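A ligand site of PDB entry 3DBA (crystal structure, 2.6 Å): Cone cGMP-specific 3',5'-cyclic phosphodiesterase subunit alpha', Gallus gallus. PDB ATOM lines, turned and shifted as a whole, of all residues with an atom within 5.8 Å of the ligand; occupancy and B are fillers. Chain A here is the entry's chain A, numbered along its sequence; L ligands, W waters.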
ATOM      1  N   ARG A  42     -25.198 -29.043  12.252  1.00  0.00           N
ATOM      2  CA  ARG A  42     -25.600 -28.244  13.403  1.00  0.00           C
ATOM      3  C   ARG A  42     -26.993 -27.677  13.203  1.00  0.00           C
ATOM      4  O   ARG A  42     -27.521 -27.668  12.091  1.00  0.00           O
ATOM      5  CB  ARG A  42     -24.636 -27.094  13.624  1.00  0.00           C
ATOM      6  CG  ARG A  42     -24.510 -26.153  12.433  1.00  0.00           C
ATOM      7  CD  ARG A  42     -23.175 -25.403  12.445  1.00  0.00           C
ATOM      8  NE  ARG A  42     -22.042 -26.313  12.348  1.00  0.00           N
ATOM      9  CZ  ARG A  42     -20.803 -26.034  12.739  1.00  0.00           C
ATOM     10  NH1 ARG A  42     -20.513 -24.847  13.281  1.00  0.00           N
ATOM     11  NH2 ARG A  42     -19.835 -26.941  12.594  1.00  0.00           N
ATOM     12  N   CYS A  43     -27.584 -27.234  14.309  1.00  0.00           N
ATOM     13  CA  CYS A  43     -28.790 -26.437  14.255  1.00  0.00           C
ATOM     14  C   CYS A  43     -28.522 -25.109  14.952  1.00  0.00           C
ATOM     15  O   CYS A  43     -27.624 -25.005  15.770  1.00  0.00           O
ATOM     16  CB  CYS A  43     -29.939 -27.145  14.962  1.00  0.00           C
ATOM     17  SG  CYS A  43     -30.222 -28.805  14.358  1.00  0.00           S
ATOM     18  N   SER A  44     -29.348 -24.120  14.632  1.00  0.00           N
ATOM     19  CA  SER A  44     -29.226 -22.791  15.191  1.00  0.00           C
ATOM     20  C   SER A  44     -30.594 -22.156  15.434  1.00  0.00           C
ATOM     21  O   SER A  44     -31.604 -22.608  14.891  1.00  0.00           O
ATOM     22  CB  SER A  44     -28.428 -21.903  14.235  1.00  0.00           C
ATOM     23  OG  SER A  44     -29.065 -21.797  12.977  1.00  0.00           O
ATOM     24  N   PHE A  46     -32.268 -18.056  15.611  1.00  0.00           N
ATOM     25  CA  PHE A  46     -32.221 -16.615  15.561  1.00  0.00           C
ATOM     26  C   PHE A  46     -33.471 -16.146  16.281  1.00  0.00           C
ATOM     27  O   PHE A  46     -34.583 -16.631  15.989  1.00  0.00           O
ATOM     28  CB  PHE A  46     -32.291 -16.092  14.132  1.00  0.00           C
ATOM     29  CG  PHE A  46     -31.050 -16.338  13.329  1.00  0.00           C
ATOM     30  CD1 PHE A  46     -30.552 -17.604  13.160  1.00  0.00           C
ATOM     31  CD2 PHE A  46     -30.405 -15.285  12.706  1.00  0.00           C
ATOM     32  CE1 PHE A  46     -29.409 -17.825  12.419  1.00  0.00           C
ATOM     33  CE2 PHE A  46     -29.273 -15.501  11.969  1.00  0.00           C
ATOM     34  CZ  PHE A  46     -28.779 -16.774  11.821  1.00  0.00           C
ATOM     35  N   LEU A  61     -28.623 -18.871  19.405  1.00  0.00           N
ATOM     36  CA  LEU A  61     -27.975 -20.173  19.562  1.00  0.00           C
ATOM     37  C   LEU A  61     -27.320 -20.559  18.227  1.00  0.00           C
ATOM     38  O   LEU A  61     -28.007 -20.729  17.209  1.00  0.00           O
ATOM     39  CB  LEU A  61     -28.987 -21.275  19.948  1.00  0.00           C
ATOM     40  CG  LEU A  61     -29.729 -21.229  21.282  1.00  0.00           C
ATOM     41  CD1 LEU A  61     -30.618 -22.438  21.412  1.00  0.00           C
ATOM     42  CD2 LEU A  61     -28.765 -21.135  22.474  1.00  0.00           C
ATOM     43  N   LEU A  62     -25.997 -20.718  18.226  1.00  0.00           N
ATOM     44  CA  LEU A  62     -25.297 -21.229  17.060  1.00  0.00           C
ATOM     45  C   LEU A  62     -24.573 -22.518  17.391  1.00  0.00           C
ATOM     46  O   LEU A  62     -24.200 -22.769  18.543  1.00  0.00           O
ATOM     47  CB  LEU A  62     -24.272 -20.213  16.547  1.00  0.00           C
ATOM     48  CG  LEU A  62     -24.772 -18.801  16.276  1.00  0.00           C
ATOM     49  CD1 LEU A  62     -23.613 -17.807  16.209  1.00  0.00           C
ATOM     50  CD2 LEU A  62     -25.607 -18.782  15.016  1.00  0.00           C
ATOM     51  N   ASN A  63     -24.348 -23.329  16.355  1.00  0.00           N
ATOM     52  CA  ASN A  63     -23.484 -24.489  16.455  1.00  0.00           C
ATOM     53  C   ASN A  63     -23.968 -25.503  17.475  1.00  0.00           C
ATOM     54  O   ASN A  63     -23.181 -26.087  18.230  1.00  0.00           O
ATOM     55  CB  ASN A  63     -22.064 -24.021  16.750  1.00  0.00           C
ATOM     56  CG  ASN A  63     -21.656 -22.877  15.853  1.00  0.00           C
ATOM     57  OD1 ASN A  63     -22.102 -22.810  14.725  1.00  0.00           O
ATOM     58  ND2 ASN A  63     -20.854 -21.972  16.352  1.00  0.00           N
ATOM     59  N   VAL A  64     -25.281 -25.740  17.468  1.00  0.00           N
ATOM     60  CA  VAL A  64     -25.871 -26.721  18.345  1.00  0.00           C
ATOM     61  C   VAL A  64     -25.698 -28.107  17.713  1.00  0.00           C
ATOM     62  O   VAL A  64     -25.867 -28.299  16.526  1.00  0.00           O
ATOM     63  CB  VAL A  64     -27.332 -26.394  18.653  1.00  0.00           C
ATOM     64  CG1 VAL A  64     -27.825 -27.251  19.803  1.00  0.00           C
ATOM     65  CG2 VAL A  64     -27.442 -24.919  18.999  1.00  0.00           C
ATOM     66  N   PHE A  83     -29.769  -8.827  11.713  1.00  0.00           N
ATOM     67  CA  PHE A  83     -30.112  -8.654  10.295  1.00  0.00           C
ATOM     68  C   PHE A  83     -31.453  -7.945  10.187  1.00  0.00           C
ATOM     69  O   PHE A  83     -32.354  -8.231  10.977  1.00  0.00           O
ATOM     70  CB  PHE A  83     -30.266 -10.016   9.605  1.00  0.00           C
ATOM     71  CG  PHE A  83     -28.986 -10.785   9.488  1.00  0.00           C
ATOM     72  CD1 PHE A  83     -28.581 -11.632  10.503  1.00  0.00           C
ATOM     73  CD2 PHE A  83     -28.163 -10.627   8.378  1.00  0.00           C
ATOM     74  CE1 PHE A  83     -27.373 -12.330  10.411  1.00  0.00           C
ATOM     75  CE2 PHE A  83     -26.964 -11.318   8.278  1.00  0.00           C
ATOM     76  CZ  PHE A  83     -26.568 -12.166   9.291  1.00  0.00           C
ATOM     77  N   ILE A  87     -32.443  -8.993   4.444  1.00  0.00           N
ATOM     78  CA  ILE A  87     -31.114  -9.585   4.275  1.00  0.00           C
ATOM     79  C   ILE A  87     -31.065 -10.972   4.926  1.00  0.00           C
ATOM     80  O   ILE A  87     -31.305 -11.099   6.127  1.00  0.00           O
ATOM     81  CB  ILE A  87     -30.022  -8.711   4.910  1.00  0.00           C
ATOM     82  CG1 ILE A  87     -29.814  -7.431   4.096  1.00  0.00           C
ATOM     83  CG2 ILE A  87     -28.725  -9.488   5.013  1.00  0.00           C
ATOM     84  CD1 ILE A  87     -28.814  -6.457   4.697  1.00  0.00           C
ATOM     85  N   GLY A  88     -30.765 -12.001   4.152  1.00  0.00           N
ATOM     86  CA  GLY A  88     -30.631 -13.347   4.679  1.00  0.00           C
ATOM     87  C   GLY A  88     -31.843 -14.242   4.473  1.00  0.00           C
ATOM     88  O   GLY A  88     -32.989 -13.766   4.398  1.00  0.00           O
ATOM     89  N   ILE A  89     -31.594 -15.553   4.388  1.00  0.00           N
ATOM     90  CA  ILE A  89     -32.657 -16.529   4.382  1.00  0.00           C
ATOM     91  C   ILE A  89     -33.390 -16.490   5.724  1.00  0.00           C
ATOM     92  O   ILE A  89     -34.616 -16.651   5.768  1.00  0.00           O
ATOM     93  CB  ILE A  89     -32.146 -17.973   4.118  1.00  0.00           C
ATOM     94  CG1 ILE A  89     -31.338 -18.029   2.812  1.00  0.00           C
ATOM     95  CG2 ILE A  89     -33.332 -18.951   4.065  1.00  0.00           C
ATOM     96  CD1 ILE A  89     -30.974 -19.428   2.355  1.00  0.00           C
ATOM     97  N   ALA A  90     -32.654 -16.311   6.802  1.00  0.00           N
ATOM     98  CA  ALA A  90     -33.253 -16.246   8.130  1.00  0.00           C
ATOM     99  C   ALA A  90     -34.256 -15.102   8.159  1.00  0.00           C
ATOM    100  O   ALA A  90     -35.405 -15.287   8.579  1.00  0.00           O
ATOM    101  CB  ALA A  90     -32.187 -16.053   9.189  1.00  0.00           C
ATOM    102  N   GLY A  91     -33.823 -13.926   7.724  1.00  0.00           N
ATOM    103  CA  GLY A  91     -34.698 -12.761   7.673  1.00  0.00           C
ATOM    104  C   GLY A  91     -35.855 -12.966   6.709  1.00  0.00           C
ATOM    105  O   GLY A  91     -36.965 -12.472   6.946  1.00  0.00           O
ATOM    106  N   HIS A 110     -31.385 -14.126  -1.412  1.00  0.00           N
ATOM    107  CA  HIS A 110     -31.785 -14.106   0.011  1.00  0.00           C
ATOM    108  C   HIS A 110     -30.613 -14.547   0.838  1.00  0.00           C
ATOM    109  O   HIS A 110     -30.317 -13.933   1.853  1.00  0.00           O
ATOM    110  CB  HIS A 110     -32.977 -14.988   0.396  1.00  0.00           C
ATOM    111  CG  HIS A 110     -34.257 -14.626  -0.277  1.00  0.00           C
ATOM    112  ND1 HIS A 110     -34.685 -13.314  -0.410  1.00  0.00           N
ATOM    113  CD2 HIS A 110     -35.220 -15.393  -0.837  1.00  0.00           C
ATOM    114  CE1 HIS A 110     -35.854 -13.307  -1.045  1.00  0.00           C
ATOM    115  NE2 HIS A 110     -36.198 -14.553  -1.311  1.00  0.00           N
ATOM    116  N   PHE A 111     -29.926 -15.616   0.430  1.00  0.00           N
ATOM    117  CA  PHE A 111     -28.762 -16.048   1.191  1.00  0.00           C
ATOM    118  C   PHE A 111     -27.830 -14.872   1.407  1.00  0.00           C
ATOM    119  O   PHE A 111     -27.522 -14.153   0.457  1.00  0.00           O
ATOM    120  CB  PHE A 111     -27.996 -17.192   0.528  1.00  0.00           C
ATOM    121  CG  PHE A 111     -26.752 -17.582   1.286  1.00  0.00           C
ATOM    122  CD1 PHE A 111     -25.504 -17.468   0.709  1.00  0.00           C
ATOM    123  CD2 PHE A 111     -26.845 -18.050   2.591  1.00  0.00           C
ATOM    124  CE1 PHE A 111     -24.357 -17.815   1.427  1.00  0.00           C
ATOM    125  CE2 PHE A 111     -25.719 -18.398   3.306  1.00  0.00           C
ATOM    126  CZ  PHE A 111     -24.467 -18.283   2.715  1.00  0.00           C
ATOM    127  N   SER A 112     -27.432 -14.665   2.672  1.00  0.00           N
ATOM    128  CA  SER A 112     -26.421 -13.681   3.073  1.00  0.00           C
ATOM    129  C   SER A 112     -25.217 -14.427   3.607  1.00  0.00           C
ATOM    130  O   SER A 112     -25.343 -15.250   4.508  1.00  0.00           O
ATOM    131  CB  SER A 112     -26.956 -12.779   4.188  1.00  0.00           C
ATOM    132  OG  SER A 112     -25.907 -12.020   4.779  1.00  0.00           O
ATOM    133  N   ASP A 113     -24.037 -14.108   3.085  1.00  0.00           N
ATOM    134  CA  ASP A 113     -22.817 -14.797   3.474  1.00  0.00           C
ATOM    135  C   ASP A 113     -22.057 -14.070   4.582  1.00  0.00           C
ATOM    136  O   ASP A 113     -20.898 -14.389   4.835  1.00  0.00           O
ATOM    137  CB  ASP A 113     -21.920 -15.018   2.248  1.00  0.00           C
ATOM    138  CG  ASP A 113     -21.373 -13.719   1.663  1.00  0.00           C
ATOM    139  OD1 ASP A 113     -21.889 -12.618   1.977  1.00  0.00           O
ATOM    140  OD2 ASP A 113     -20.412 -13.797   0.864  1.00  0.00           O
ATOM    141  N   LEU A 115     -22.347 -14.017   7.974  1.00  0.00           N
ATOM    142  CA  LEU A 115     -21.944 -14.861   9.098  1.00  0.00           C
ATOM    143  C   LEU A 115     -20.864 -15.862   8.695  1.00  0.00           C
ATOM    144  O   LEU A 115     -19.982 -16.177   9.492  1.00  0.00           O
ATOM    145  CB  LEU A 115     -23.125 -15.597   9.724  1.00  0.00           C
ATOM    146  CG  LEU A 115     -23.760 -14.957  10.970  1.00  0.00           C
ATOM    147  CD1 LEU A 115     -24.990 -15.781  11.416  1.00  0.00           C
ATOM    148  CD2 LEU A 115     -22.763 -14.794  12.123  1.00  0.00           C
ATOM    149  N   ASP A 116     -20.937 -16.385   7.463  1.00  0.00           N
ATOM    150  CA  ASP A 116     -19.934 -17.317   6.962  1.00  0.00           C
ATOM    151  C   ASP A 116     -18.559 -16.634   6.950  1.00  0.00           C
ATOM    152  O   ASP A 116     -17.562 -17.235   7.349  1.00  0.00           O
ATOM    153  CB  ASP A 116     -20.313 -17.837   5.575  1.00  0.00           C
ATOM    154  CG  ASP A 116     -21.204 -19.085   5.630  1.00  0.00           C
ATOM    155  OD1 ASP A 116     -21.956 -19.288   6.607  1.00  0.00           O
ATOM    156  OD2 ASP A 116     -21.150 -19.878   4.669  1.00  0.00           O
ATOM    157  N   THR A 119     -17.653 -15.924  10.957  1.00  0.00           N
ATOM    158  CA  THR A 119     -17.373 -17.141  11.723  1.00  0.00           C
ATOM    159  C   THR A 119     -16.382 -18.109  11.043  1.00  0.00           C
ATOM    160  O   THR A 119     -15.755 -18.930  11.722  1.00  0.00           O
ATOM    161  CB  THR A 119     -18.660 -17.919  11.985  1.00  0.00           C
ATOM    162  OG1 THR A 119     -19.230 -18.304  10.726  1.00  0.00           O
ATOM    163  CG2 THR A 119     -19.652 -17.061  12.752  1.00  0.00           C
ATOM    164  N   TYR A 121     -17.373 -20.419   8.956  1.00  0.00           N
ATOM    165  CA  TYR A 121     -18.152 -21.612   8.603  1.00  0.00           C
ATOM    166  C   TYR A 121     -18.667 -21.566   7.171  1.00  0.00           C
ATOM    167  O   TYR A 121     -19.022 -20.495   6.671  1.00  0.00           O
ATOM    168  CB  TYR A 121     -19.362 -21.724   9.536  1.00  0.00           C
ATOM    169  CG  TYR A 121     -20.205 -22.973   9.356  1.00  0.00           C
ATOM    170  CD1 TYR A 121     -19.650 -24.240   9.509  1.00  0.00           C
ATOM    171  CD2 TYR A 121     -21.573 -22.875   9.054  1.00  0.00           C
ATOM    172  CE1 TYR A 121     -20.433 -25.392   9.354  1.00  0.00           C
ATOM    173  CE2 TYR A 121     -22.339 -24.005   8.910  1.00  0.00           C
ATOM    174  CZ  TYR A 121     -21.765 -25.263   9.062  1.00  0.00           C
ATOM    175  OH  TYR A 121     -22.541 -26.394   8.916  1.00  0.00           O
ATOM    176  N   THR A 123     -21.685 -22.616   4.876  1.00  0.00           N
ATOM    177  CA  THR A 123     -23.071 -23.072   4.856  1.00  0.00           C
ATOM    178  C   THR A 123     -23.400 -23.530   3.453  1.00  0.00           C
ATOM    179  O   THR A 123     -23.155 -22.802   2.505  1.00  0.00           O
ATOM    180  CB  THR A 123     -24.041 -21.939   5.224  1.00  0.00           C
ATOM    181  OG1 THR A 123     -23.579 -21.283   6.412  1.00  0.00           O
ATOM    182  CG2 THR A 123     -25.428 -22.490   5.444  1.00  0.00           C
ATOM    183  N   MET A 126     -29.823 -26.231   3.937  1.00  0.00           N
ATOM    184  CA  MET A 126     -30.503 -25.653   5.076  1.00  0.00           C
ATOM    185  C   MET A 126     -31.983 -25.947   5.061  1.00  0.00           C
ATOM    186  O   MET A 126     -32.615 -25.919   4.001  1.00  0.00           O
ATOM    187  CB  MET A 126     -30.309 -24.144   5.031  1.00  0.00           C
ATOM    188  CG  MET A 126     -30.855 -23.401   6.207  1.00  0.00           C
ATOM    189  SD  MET A 126     -30.438 -21.662   6.041  1.00  0.00           S
ATOM    190  CE  MET A 126     -31.723 -21.203   4.917  1.00  0.00           C
ATOM    191  N   MET A 142     -33.018 -23.228  12.311  1.00  0.00           N
ATOM    192  CA  MET A 142     -32.529 -23.969  11.160  1.00  0.00           C
ATOM    193  C   MET A 142     -31.605 -25.148  11.474  1.00  0.00           C
ATOM    194  O   MET A 142     -30.908 -25.155  12.504  1.00  0.00           O
ATOM    195  CB  MET A 142     -31.896 -23.048  10.100  1.00  0.00           C
ATOM    196  CG  MET A 142     -31.171 -21.842  10.565  1.00  0.00           C
ATOM    197  SD  MET A 142     -30.864 -20.666   9.208  1.00  0.00           S
ATOM    198  CE  MET A 142     -30.715 -19.189  10.178  1.00  0.00           C
ATOM    199  N   LEU A 144     -28.520 -26.943   9.596  1.00  0.00           N
ATOM    200  CA  LEU A 144     -27.575 -26.685   8.553  1.00  0.00           C
ATOM    201  C   LEU A 144     -26.799 -27.947   8.181  1.00  0.00           C
ATOM    202  O   LEU A 144     -26.608 -28.832   9.006  1.00  0.00           O
ATOM    203  CB  LEU A 144     -26.624 -25.595   9.007  1.00  0.00           C
ATOM    204  CG  LEU A 144     -27.264 -24.254   9.288  1.00  0.00           C
ATOM    205  CD1 LEU A 144     -26.185 -23.282   9.760  1.00  0.00           C
ATOM    206  CD2 LEU A 144     -27.894 -23.721   8.042  1.00  0.00           C
HETATM  207  P1  LIG L   1     -28.754 -16.746   5.980  1.00  0.00           P
HETATM  208  O1  LIG L   1     -28.707 -16.340   4.525  1.00  0.00           O
HETATM  209  O2  LIG L   1     -30.063 -17.132   6.652  1.00  0.00           O
HETATM  210  O3  LIG L   1     -28.152 -15.539   6.839  1.00  0.00           O
HETATM  211  C1  LIG L   1     -27.761 -15.755   8.186  1.00  0.00           C
HETATM  212  C2  LIG L   1     -26.760 -16.892   8.163  1.00  0.00           C
HETATM  213  O4  LIG L   1     -26.277 -17.359   9.405  1.00  0.00           O
HETATM  214  C3  LIG L   1     -27.367 -18.140   7.590  1.00  0.00           C
HETATM  215  O5  LIG L   1     -27.696 -17.912   6.235  1.00  0.00           O
HETATM  216  C4  LIG L   1     -26.248 -19.123   7.832  1.00  0.00           C
HETATM  217  O6  LIG L   1     -25.343 -19.085   6.717  1.00  0.00           O
HETATM  218  C5  LIG L   1     -25.635 -18.601   9.130  1.00  0.00           C
HETATM  219  N1  LIG L   1     -25.887 -19.549  10.237  1.00  0.00           N
HETATM  220  C6  LIG L   1     -27.083 -20.001  10.682  1.00  0.00           C
HETATM  221  N2  LIG L   1     -26.903 -20.881  11.708  1.00  0.00           N
HETATM  222  C7  LIG L   1     -25.578 -20.993  11.927  1.00  0.00           C
HETATM  223  C8  LIG L   1     -24.697 -21.746  12.836  1.00  0.00           C
HETATM  224  O7  LIG L   1     -25.146 -22.516  13.696  1.00  0.00           O
HETATM  225  N3  LIG L   1     -23.374 -21.560  12.711  1.00  0.00           N
HETATM  226  C9  LIG L   1     -22.833 -20.737  11.786  1.00  0.00           C
HETATM  227  N4  LIG L   1     -21.496 -20.623  11.718  1.00  0.00           N
HETATM  228  N5  LIG L   1     -23.585 -20.032  10.915  1.00  0.00           N
HETATM  229  C10 LIG L   1     -24.917 -20.123  10.950  1.00  0.00           C
HETATM  230  O   HOH W   1     -19.922 -20.233  14.498  1.00  0.00           O
HETATM  231  O   HOH W   2     -21.491 -18.822   9.426  1.00  0.00           O
HETATM  232  O   HOH W   3     -23.353 -16.751   6.162  1.00  0.00           O
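The backbone NH (N) of Ser 112 lies within hydrogen-bond range of an oxygen (O1) of the ligand (2.8 Å). OG of Ser 44 lies within hydrogen-bond range of N2 of the ligand (2.7 Å). The side-chain hydroxyl of Thr 123 is in hydrogen-bond range of an oxygen (O6) of the ligand (2.8 Å). The backbone NH of Ile 89 sits at hydrogen-bond distance from an oxygen (O1) of the ligand (3.0 Å). O6 of the ligand sits at hydrogen-bond distance from OD1 of Asp 116 (3.4 Å). A nitrogen (N3) of the ligand lies within hydrogen-bond range of the side-chain amide oxygen of Asn 63 (2.7 Å). N of Ala 90 is in hydrogen-bond range of O2 of the ligand (2.7 Å). The side-chain hydroxyl (OG1) of Thr 119 is in hydrogen-bond range of a nitrogen (N4) of the ligand (3.4 Å). An oxygen (O7) of the ligand sits at hydrogen-bond distance from the backbone NH of Asn 63 (2.9 Å).
The backbone carbonyl oxygen (O) of Leu 115 is in hydrogen-bond range of the side-chain hydroxyl (OG1) of Thr 119 (2.6 Å). N of Ser 44 sits at hydrogen-bond distance from O of Met 142 (2.8 Å). N of Leu 144 sits at hydrogen-bond distance from O of Arg 42 (2.8 Å). NE of Arg 42 lies close to OH of Tyr 121 (3.5 Å). The backbone NH (N) of Gly 88 lies close to the backbone carbonyl oxygen (O) of His 110 (3.0 Å). The backbone NH (N) of Tyr 121 lies close to the side-chain hydroxyl (OG1) of Thr 119 (3.3 Å). The backbone NH (N) of Ile 89 sits at hydrogen-bond distance from the backbone carbonyl oxygen (O) of His 110, at 3.3 Å. The side-chain amide oxygen of Asn 63 is in hydrogen-bond range of the guanidinium group of Arg 42, 3.0 Å away.
Arg 42 touches the ligand. CZ of Phe 46 touches O4 of the ligand, 3.5 Å away. Leu 62 touches the ligand. Phe 83 touches the ligand. CA of Gly 88 touches O1 of the ligand, 3.6 Å away. His 110 touches the ligand. Phe 111 touches the ligand (CD2 to O1, 3.2 Å). Leu 115 touches the ligand. Tyr 121 touches the ligand (CB to N4, 3.2 Å). Met 142 touches the ligand. CD1 of Leu 144 touches N2 of the ligand (3.2 Å). Hydrophobic or aromatic side chains that line the ligand: Phe 46, Leu 62, Phe 83, Ile 89, Ala 90, Phe 111, Leu 115, Tyr 121, Met 142 and Leu 144. 19 residues have an atom within 4 Å of the ligand: Arg 42, Ser 44, Phe 46, Leu 62, Asn 63, Phe 83, Gly 88, Ile 89, Ala 90, His 110, Phe 111, Ser 112, Leu 115, Asp 116, Thr 119, Tyr 121, Thr 123, Met 142 and Leu 144. The nearest printed residue that does not touch the ligand is Cys 43 (4.1 Å).
Water W3 lies within hydrogen-bond range of N of Asp 116 (2.8 Å), O of Ser 112 (3.0 Å), O6 of the ligand (3.1 Å) and N of Leu 115 (3.4 Å). Water W1 bridges the side-chain amide nitrogen (ND2) of Asn 63 (2.7 Å) and a nitrogen (N4) of the ligand (3.2 Å).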
